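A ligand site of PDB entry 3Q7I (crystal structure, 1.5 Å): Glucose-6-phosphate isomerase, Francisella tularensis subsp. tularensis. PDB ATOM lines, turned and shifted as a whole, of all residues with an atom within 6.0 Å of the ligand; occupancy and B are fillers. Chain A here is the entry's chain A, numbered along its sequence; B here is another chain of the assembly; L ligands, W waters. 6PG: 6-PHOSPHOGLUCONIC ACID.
NH2 of Arg 264 lies within salt-bridge range of OE2 of Glu 349, 3.2 Å away. The side-chain carboxylate (OE1) of Glu 349 sits at hydrogen-bond distance from the side-chain amide nitrogen (NE2) of Gln 345. OG1 of Thr 206 sits at hydrogen-bond distance from OG of Ser 203 (3.3 Å). OG of Ser 203 sits close to N of Ser 205, 3.2 Å away. The side-chain hydroxyl (OG) of Ser 151 sits close to the backbone carbonyl oxygen (O) of Ala 200, at 3.5 Å. The guanidinium group of Arg 264 sits at hydrogen-bond distance from the side-chain amide oxygen of Gln 501. The side-chain amide nitrogen (NE2) of Gln 345 sits close to the backbone NH (N) of Gly 150 (3.3 Å). OE2 of Glu 505 sits at hydrogen-bond distance from NE2 of Gln 501, 2.9 Å away.
Water W4 lies within hydrogen-bond range of the side-chain hydroxyl of Thr 209 (2.7 Å), an oxygen (O2P) of the ligand (2.7 Å), the backbone carbonyl oxygen of Ala 200 (2.8 Å) and the backbone NH of Ile 148 (3.1 Å). Water W3 lies within hydrogen-bond range of an oxygen (O1A) of the ligand, the side-chain amide oxygen of Gln 501, the backbone NH of Gly 263 and the guanidinium group of Arg 264.
OE1 of Glu 349 sits close to O1 of the ligand (2.5 Å). O of His 380 of chain B sits at hydrogen-bond distance from O3 of the ligand (2.6 Å). A ring nitrogen (ND1) of His 380 of chain B is in hydrogen-bond range of an oxygen (O5) of the ligand, 2.7 Å away. An oxygen (O2P) of the ligand lies within hydrogen-bond range of the side-chain hydroxyl (OG) of Ser 201 (2.7 Å). An oxygen (O2P) of the ligand sits at hydrogen-bond distance from the side-chain hydroxyl (OG1) of Thr 206 (2.7 Å). An oxygen (O3P) of the ligand lies within hydrogen-bond range of the backbone NH of Ser 203 (2.8 Å). The side-chain hydroxyl (OG) of Ser 203 lies within hydrogen-bond range of an oxygen (O3P) of the ligand (2.7 Å). An oxygen (O3P) of the ligand is in salt-bridge range of the side-chain amino group (NZ) of Lys 508, at 3.9 Å. The side-chain hydroxyl of Ser 151 is in hydrogen-bond range of an oxygen (O1P) of the ligand (2.8 Å). N of Lys 202 lies within hydrogen-bond range of O1P of the ligand, 2.8 Å away. The backbone NH of Gly 263 is in hydrogen-bond range of an oxygen (O1A) of the ligand, 2.9 Å away. The backbone NH (N) of Arg 264 is in hydrogen-bond range of an oxygen (O1A) of the ligand (2.9 Å). The guanidinium group of Arg 264 lies within salt-bridge range of an oxygen (O1) of the ligand, at 3.4 Å. The backbone NH (N) of Gly 150 lies within hydrogen-bond range of an oxygen (O4) of the ligand (3.0 Å). The side-chain amide nitrogen (NE2) of Gln 345 is in hydrogen-bond range of an oxygen (O1) of the ligand, at 3.0 Å.
Merely in contact with the ligand: Ile 148, Gly 149, Gln 501 and Gly 262. Within 4 Å of the ligand: Ile 148, Gly 149, Gly 150, Ser 151, Ser 201, Lys 202, Ser 203, Thr 206, Gly 262, Gly 263, Arg 264, Gln 345, Glu 349, Gln 501, Lys 508 and His 380 of chain B. The nearest printed residue that does not touch the ligand is Val 504 (4.1 Å).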
ATOM      1  N   ILE A 148     -18.237  -0.937  19.223  1.00  0.00           N
ATOM      2  CA  ILE A 148     -16.846  -1.399  19.290  1.00  0.00           C
ATOM      3  C   ILE A 148     -16.330  -1.719  17.885  1.00  0.00           C
ATOM      4  O   ILE A 148     -17.132  -2.010  16.991  1.00  0.00           O
ATOM      5  CB  ILE A 148     -16.663  -2.593  20.264  1.00  0.00           C
ATOM      6  CG1 ILE A 148     -15.196  -2.872  20.679  1.00  0.00           C
ATOM      7  CG2 ILE A 148     -17.441  -3.830  19.779  1.00  0.00           C
ATOM      8  CD1 ILE A 148     -15.102  -3.708  21.952  1.00  0.00           C
ATOM      9  N   GLY A 149     -15.013  -1.713  17.697  1.00  0.00           N
ATOM     10  CA  GLY A 149     -14.450  -2.044  16.399  1.00  0.00           C
ATOM     11  C   GLY A 149     -14.868  -1.055  15.322  1.00  0.00           C
ATOM     12  O   GLY A 149     -14.745   0.155  15.463  1.00  0.00           O
ATOM     13  N   GLY A 150     -15.420  -1.588  14.268  1.00  0.00           N
ATOM     14  CA  GLY A 150     -15.926  -0.744  13.189  1.00  0.00           C
ATOM     15  C   GLY A 150     -16.994   0.231  13.593  1.00  0.00           C
ATOM     16  O   GLY A 150     -17.220   1.220  12.925  1.00  0.00           O
ATOM     17  N   SER A 151     -17.705  -0.050  14.693  1.00  0.00           N
ATOM     18  CA  SER A 151     -18.719   0.851  15.212  1.00  0.00           C
ATOM     19  C   SER A 151     -18.226   1.849  16.225  1.00  0.00           C
ATOM     20  O   SER A 151     -19.033   2.529  16.875  1.00  0.00           O
ATOM     21  CB  SER A 151     -19.864   0.019  15.785  1.00  0.00           C
ATOM     22  OG  SER A 151     -20.557  -0.626  14.670  1.00  0.00           O
ATOM     23  N   ALA A 200     -24.453   1.799  18.408  1.00  0.00           N
ATOM     24  CA  ALA A 200     -23.937   1.605  17.035  1.00  0.00           C
ATOM     25  C   ALA A 200     -23.569   0.150  16.929  1.00  0.00           C
ATOM     26  O   ALA A 200     -22.563  -0.269  17.507  1.00  0.00           O
ATOM     27  CB  ALA A 200     -22.713   2.538  16.833  1.00  0.00           C
ATOM     28  N   SER A 201     -24.378  -0.618  16.192  1.00  0.00           N
ATOM     29  CA  SER A 201     -24.056  -2.033  16.026  1.00  0.00           C
ATOM     30  C   SER A 201     -24.732  -2.602  14.794  1.00  0.00           C
ATOM     31  O   SER A 201     -25.952  -2.761  14.762  1.00  0.00           O
ATOM     32  CB  SER A 201     -24.479  -2.820  17.247  1.00  0.00           C
ATOM     33  OG  SER A 201     -24.153  -4.189  17.145  1.00  0.00           O
ATOM     34  N   LYS A 202     -23.914  -2.925  13.809  1.00  0.00           N
ATOM     35  CA  LYS A 202     -24.428  -3.516  12.562  1.00  0.00           C
ATOM     36  C   LYS A 202     -25.223  -4.728  12.856  1.00  0.00           C
ATOM     37  O   LYS A 202     -26.353  -4.873  12.345  1.00  0.00           O
ATOM     38  CB  LYS A 202     -23.247  -3.830  11.647  1.00  0.00           C
ATOM     39  CG  LYS A 202     -23.665  -4.393  10.287  1.00  0.00           C
ATOM     40  CD  LYS A 202     -22.470  -4.722   9.412  1.00  0.00           C
ATOM     41  CE  LYS A 202     -22.900  -5.325   8.071  1.00  0.00           C
ATOM     42  NZ  LYS A 202     -21.667  -5.589   7.200  1.00  0.00           N
ATOM     43  N   SER A 203     -24.688  -5.622  13.651  1.00  0.00           N
ATOM     44  CA  SER A 203     -25.370  -6.892  13.975  1.00  0.00           C
ATOM     45  C   SER A 203     -26.408  -6.805  15.075  1.00  0.00           C
ATOM     46  O   SER A 203     -27.291  -7.664  15.207  1.00  0.00           O
ATOM     47  CB  SER A 203     -24.332  -7.926  14.407  1.00  0.00           C
ATOM     48  OG  SER A 203     -23.675  -7.574  15.625  1.00  0.00           O
ATOM     49  N   PHE A 204     -26.266  -5.831  15.968  1.00  0.00           N
ATOM     50  CA  PHE A 204     -27.005  -5.702  17.174  1.00  0.00           C
ATOM     51  C   PHE A 204     -26.867  -6.912  18.097  1.00  0.00           C
ATOM     52  O   PHE A 204     -27.748  -7.173  18.916  1.00  0.00           O
ATOM     53  CB  PHE A 204     -28.502  -5.315  16.953  1.00  0.00           C
ATOM     54  CG  PHE A 204     -28.916  -4.103  17.771  1.00  0.00           C
ATOM     55  CD1 PHE A 204     -28.379  -2.893  17.440  1.00  0.00           C
ATOM     56  CD2 PHE A 204     -29.749  -4.193  18.863  1.00  0.00           C
ATOM     57  CE1 PHE A 204     -28.654  -1.725  18.190  1.00  0.00           C
ATOM     58  CE2 PHE A 204     -30.076  -3.020  19.601  1.00  0.00           C
ATOM     59  CZ  PHE A 204     -29.481  -1.823  19.231  1.00  0.00           C
ATOM     60  N   SER A 205     -25.755  -7.650  18.019  1.00  0.00           N
ATOM     61  CA  SER A 205     -25.566  -8.767  18.938  1.00  0.00           C
ATOM     62  C   SER A 205     -24.152  -8.918  19.497  1.00  0.00           C
ATOM     63  O   SER A 205     -23.771  -9.976  20.026  1.00  0.00           O
ATOM     64  CB  SER A 205     -25.975 -10.071  18.307  1.00  0.00           C
ATOM     65  OG  SER A 205     -25.251 -10.300  17.150  1.00  0.00           O
ATOM     66  N   THR A 206     -23.398  -7.837  19.477  1.00  0.00           N
ATOM     67  CA  THR A 206     -21.997  -7.885  19.910  1.00  0.00           C
ATOM     68  C   THR A 206     -21.972  -7.776  21.428  1.00  0.00           C
ATOM     69  O   THR A 206     -22.608  -6.880  21.975  1.00  0.00           O
ATOM     70  CB  THR A 206     -21.250  -6.730  19.294  1.00  0.00           C
ATOM     71  OG1 THR A 206     -21.303  -6.869  17.867  1.00  0.00           O
ATOM     72  CG2 THR A 206     -19.762  -6.705  19.731  1.00  0.00           C
ATOM     73  N   THR A 209     -21.068  -4.357  23.269  1.00  0.00           N
ATOM     74  CA  THR A 209     -22.034  -3.310  23.008  1.00  0.00           C
ATOM     75  C   THR A 209     -23.373  -3.646  23.712  1.00  0.00           C
ATOM     76  O   THR A 209     -23.984  -2.753  24.234  1.00  0.00           O
ATOM     77  CB  THR A 209     -22.186  -3.152  21.521  1.00  0.00           C
ATOM     78  OG1 THR A 209     -20.915  -2.831  20.964  1.00  0.00           O
ATOM     79  CG2 THR A 209     -23.198  -2.007  21.201  1.00  0.00           C
ATOM     80  N   MET A 257     -27.986   0.842   8.358  1.00  0.00           N
ATOM     81  CA  MET A 257     -26.871   0.532   7.474  1.00  0.00           C
ATOM     82  C   MET A 257     -27.187  -0.834   6.846  1.00  0.00           C
ATOM     83  O   MET A 257     -28.183  -1.441   7.143  1.00  0.00           O
ATOM     84  CB  MET A 257     -25.568   0.520   8.256  1.00  0.00           C
ATOM     85  CG  MET A 257     -25.434  -0.653   9.235  1.00  0.00           C
ATOM     86  SD  MET A 257     -24.152  -0.312  10.500  1.00  0.00           S
ATOM     87  CE  MET A 257     -22.637  -0.572   9.437  1.00  0.00           C
ATOM     88  N   GLY A 262     -19.046  -2.871   5.331  1.00  0.00           N
ATOM     89  CA  GLY A 262     -18.194  -3.537   6.324  1.00  0.00           C
ATOM     90  C   GLY A 262     -17.960  -2.617   7.506  1.00  0.00           C
ATOM     91  O   GLY A 262     -17.839  -1.403   7.298  1.00  0.00           O
ATOM     92  N   GLY A 263     -17.927  -3.174   8.736  1.00  0.00           N
ATOM     93  CA  GLY A 263     -17.722  -2.339   9.927  1.00  0.00           C
ATOM     94  C   GLY A 263     -16.500  -1.411   9.798  1.00  0.00           C
ATOM     95  O   GLY A 263     -16.494  -0.192  10.050  1.00  0.00           O
ATOM     96  N   ARG A 264     -15.371  -1.985   9.342  1.00  0.00           N
ATOM     97  CA  ARG A 264     -14.126  -1.244   9.197  1.00  0.00           C
ATOM     98  C   ARG A 264     -14.082  -0.257   8.011  1.00  0.00           C
ATOM     99  O   ARG A 264     -13.073   0.445   7.821  1.00  0.00           O
ATOM    100  CB  ARG A 264     -12.907  -2.217   9.168  1.00  0.00           C
ATOM    101  CG  ARG A 264     -12.930  -3.179   7.965  1.00  0.00           C
ATOM    102  CD  ARG A 264     -11.774  -4.146   8.027  1.00  0.00           C
ATOM    103  NE  ARG A 264     -11.939  -5.300   7.136  1.00  0.00           N
ATOM    104  CZ  ARG A 264     -12.649  -6.369   7.372  1.00  0.00           C
ATOM    105  NH1 ARG A 264     -12.677  -7.328   6.478  1.00  0.00           N
ATOM    106  NH2 ARG A 264     -13.318  -6.522   8.507  1.00  0.00           N
ATOM    107  N   TYR A 265     -15.191  -0.194   7.269  1.00  0.00           N
ATOM    108  CA  TYR A 265     -15.423   0.741   6.190  1.00  0.00           C
ATOM    109  C   TYR A 265     -16.741   1.483   6.406  1.00  0.00           C
ATOM    110  O   TYR A 265     -17.373   1.915   5.453  1.00  0.00           O
ATOM    111  CB  TYR A 265     -15.476  -0.024   4.880  1.00  0.00           C
ATOM    112  CG  TYR A 265     -14.205  -0.782   4.561  1.00  0.00           C
ATOM    113  CD1 TYR A 265     -13.076  -0.139   4.113  1.00  0.00           C
ATOM    114  CD2 TYR A 265     -14.129  -2.168   4.711  1.00  0.00           C
ATOM    115  CE1 TYR A 265     -11.900  -0.811   3.859  1.00  0.00           C
ATOM    116  CE2 TYR A 265     -12.963  -2.863   4.442  1.00  0.00           C
ATOM    117  CZ  TYR A 265     -11.855  -2.170   4.041  1.00  0.00           C
ATOM    118  OH  TYR A 265     -10.636  -2.798   3.742  1.00  0.00           O
ATOM    119  N   ILE A 271     -23.284   5.110  10.745  1.00  0.00           N
ATOM    120  CA  ILE A 271     -22.343   4.914  11.855  1.00  0.00           C
ATOM    121  C   ILE A 271     -21.554   6.180  12.108  1.00  0.00           C
ATOM    122  O   ILE A 271     -21.132   6.454  13.255  1.00  0.00           O
ATOM    123  CB  ILE A 271     -21.397   3.730  11.545  1.00  0.00           C
ATOM    124  CG1 ILE A 271     -22.156   2.431  11.549  1.00  0.00           C
ATOM    125  CG2 ILE A 271     -20.173   3.734  12.534  1.00  0.00           C
ATOM    126  CD1 ILE A 271     -22.627   1.961  12.976  1.00  0.00           C
ATOM    127  N   GLN A 345      -6.687  -1.532  11.969  1.00  0.00           N
ATOM    128  CA  GLN A 345      -7.857  -2.303  11.767  1.00  0.00           C
ATOM    129  C   GLN A 345      -8.185  -2.504  10.284  1.00  0.00           C
ATOM    130  O   GLN A 345      -8.400  -3.646   9.851  1.00  0.00           O
ATOM    131  CB  GLN A 345      -9.029  -1.637  12.503  1.00  0.00           C
ATOM    132  CG  GLN A 345     -10.330  -2.326  12.239  1.00  0.00           C
ATOM    133  CD  GLN A 345     -11.502  -1.946  13.163  1.00  0.00           C
ATOM    134  OE1 GLN A 345     -11.422  -1.046  13.996  1.00  0.00           O
ATOM    135  NE2 GLN A 345     -12.587  -2.676  12.991  1.00  0.00           N
ATOM    136  N   GLU A 349      -7.167  -6.411   9.561  1.00  0.00           N
ATOM    137  CA  GLU A 349      -8.383  -7.219   9.588  1.00  0.00           C
ATOM    138  C   GLU A 349      -8.820  -7.601   8.152  1.00  0.00           C
ATOM    139  O   GLU A 349      -9.424  -8.656   7.958  1.00  0.00           O
ATOM    140  CB  GLU A 349      -9.523  -6.506  10.302  1.00  0.00           C
ATOM    141  CG  GLU A 349     -10.619  -7.440  10.666  1.00  0.00           C
ATOM    142  CD  GLU A 349     -11.808  -6.748  11.299  1.00  0.00           C
ATOM    143  OE1 GLU A 349     -11.835  -5.502  11.358  1.00  0.00           O
ATOM    144  OE2 GLU A 349     -12.769  -7.474  11.557  1.00  0.00           O
ATOM    145  N   GLN A 501     -14.126 -11.664   7.839  1.00  0.00           N
ATOM    146  CA  GLN A 501     -13.270 -11.637   9.063  1.00  0.00           C
ATOM    147  C   GLN A 501     -13.613 -12.804   9.939  1.00  0.00           C
ATOM    148  O   GLN A 501     -14.107 -12.640  11.067  1.00  0.00           O
ATOM    149  CB  GLN A 501     -13.372 -10.267   9.803  1.00  0.00           C
ATOM    150  CG  GLN A 501     -14.766  -9.845  10.226  1.00  0.00           C
ATOM    151  CD  GLN A 501     -15.628  -9.314   9.102  1.00  0.00           C
ATOM    152  OE1 GLN A 501     -15.153  -8.512   8.259  1.00  0.00           O
ATOM    153  NE2 GLN A 501     -16.874  -9.754   9.057  1.00  0.00           N
ATOM    154  N   VAL A 504     -12.440 -12.646  13.551  1.00  0.00           N
ATOM    155  CA  VAL A 504     -13.230 -11.726  14.367  1.00  0.00           C
ATOM    156  C   VAL A 504     -14.614 -12.339  14.660  1.00  0.00           C
ATOM    157  O   VAL A 504     -15.152 -12.290  15.792  1.00  0.00           O
ATOM    158  CB  VAL A 504     -13.292 -10.331  13.710  1.00  0.00           C
ATOM    159  CG1 VAL A 504     -14.367  -9.439  14.374  1.00  0.00           C
ATOM    160  CG2 VAL A 504     -11.917  -9.676  13.741  1.00  0.00           C
ATOM    161  N   GLU A 505     -15.217 -12.909  13.651  1.00  0.00           N
ATOM    162  CA  GLU A 505     -16.453 -13.614  13.891  1.00  0.00           C
ATOM    163  C   GLU A 505     -16.322 -14.721  14.974  1.00  0.00           C
ATOM    164  O   GLU A 505     -17.230 -14.867  15.800  1.00  0.00           O
ATOM    165  CB  GLU A 505     -17.055 -14.149  12.590  1.00  0.00           C
ATOM    166  CG  GLU A 505     -17.314 -13.158  11.558  1.00  0.00           C
ATOM    167  CD  GLU A 505     -18.315 -12.072  11.933  1.00  0.00           C
ATOM    168  OE1 GLU A 505     -19.225 -12.264  12.787  1.00  0.00           O
ATOM    169  OE2 GLU A 505     -18.243 -11.068  11.283  1.00  0.00           O
ATOM    170  N   LYS A 508     -16.196 -13.319  18.636  1.00  0.00           N
ATOM    171  CA  LYS A 508     -17.515 -12.937  19.165  1.00  0.00           C
ATOM    172  C   LYS A 508     -18.317 -14.078  19.788  1.00  0.00           C
ATOM    173  O   LYS A 508     -19.317 -13.804  20.514  1.00  0.00           O
ATOM    174  CB  LYS A 508     -18.339 -12.340  18.045  1.00  0.00           C
ATOM    175  CG  LYS A 508     -17.780 -11.036  17.624  1.00  0.00           C
ATOM    176  CD  LYS A 508     -18.666 -10.333  16.642  1.00  0.00           C
ATOM    177  CE  LYS A 508     -18.554  -8.867  16.909  1.00  0.00           C
ATOM    178  NZ  LYS A 508     -19.396  -8.152  16.052  1.00  0.00           N
ATOM    179  N   HIS B 380     -11.671  -7.069  17.648  1.00  0.00           N
ATOM    180  CA  HIS B 380     -12.541  -6.647  16.563  1.00  0.00           C
ATOM    181  C   HIS B 380     -11.750  -6.130  15.412  1.00  0.00           C
ATOM    182  O   HIS B 380     -12.346  -5.661  14.458  1.00  0.00           O
ATOM    183  CB  HIS B 380     -13.541  -5.606  17.109  1.00  0.00           C
ATOM    184  CG  HIS B 380     -14.372  -6.175  18.203  1.00  0.00           C
ATOM    185  ND1 HIS B 380     -15.637  -6.730  17.974  1.00  0.00           N
ATOM    186  CD2 HIS B 380     -14.105  -6.372  19.522  1.00  0.00           C
ATOM    187  CE1 HIS B 380     -16.107  -7.194  19.112  1.00  0.00           C
ATOM    188  NE2 HIS B 380     -15.202  -7.014  20.067  1.00  0.00           N
ATOM    189  N   ALA B 381     -10.424  -6.232  15.497  1.00  0.00           N
ATOM    190  CA  ALA B 381      -9.631  -5.506  14.549  1.00  0.00           C
ATOM    191  C   ALA B 381      -8.473  -6.463  14.250  1.00  0.00           C
ATOM    192  O   ALA B 381      -8.623  -7.493  13.563  1.00  0.00           O
ATOM    193  CB  ALA B 381      -9.281  -4.219  15.214  1.00  0.00           C
HETATM  194  C1  6PG L   1     -15.209  -5.011  11.065  1.00  0.00           C
HETATM  195  C2  6PG L   1     -15.570  -6.084  12.042  1.00  0.00           C
HETATM  196  C3  6PG L   1     -15.734  -5.668  13.526  1.00  0.00           C
HETATM  197  C4  6PG L   1     -17.111  -5.087  13.869  1.00  0.00           C
HETATM  198  C5  6PG L   1     -17.365  -5.029  15.403  1.00  0.00           C
HETATM  199  C6  6PG L   1     -18.695  -4.416  15.805  1.00  0.00           C
HETATM  200  O1A 6PG L   1     -15.980  -4.733  10.149  1.00  0.00           O
HETATM  201  O1  6PG L   1     -14.080  -4.533  11.134  1.00  0.00           O
HETATM  202  O2  6PG L   1     -16.699  -6.896  11.614  1.00  0.00           O
HETATM  203  O3  6PG L   1     -14.751  -4.663  13.970  1.00  0.00           O
HETATM  204  O4  6PG L   1     -17.235  -3.771  13.359  1.00  0.00           O
HETATM  205  O5  6PG L   1     -17.320  -6.409  15.875  1.00  0.00           O
HETATM  206  O6  6PG L   1     -19.757  -5.185  15.184  1.00  0.00           O
HETATM  207  P   6PG L   1     -21.220  -4.600  15.275  1.00  0.00           P
HETATM  208  O1P 6PG L   1     -21.228  -3.292  14.561  1.00  0.00           O
HETATM  209  O2P 6PG L   1     -21.549  -4.476  16.739  1.00  0.00           O
HETATM  210  O3P 6PG L   1     -22.044  -5.681  14.599  1.00  0.00           O
HETATM  211  O   HOH W   1     -19.723  -3.229  12.330  1.00  0.00           O
HETATM  212  O   HOH W   2     -21.125  -7.227  12.564  1.00  0.00           O
HETATM  213  O   HOH W   3     -16.733  -6.223   7.943  1.00  0.00           O
HETATM  214  O   HOH W   4     -20.829  -2.326  18.295  1.00  0.00           O
HETATM  215  O   HOH W   5     -19.267  -5.693  11.082  1.00  0.00           O
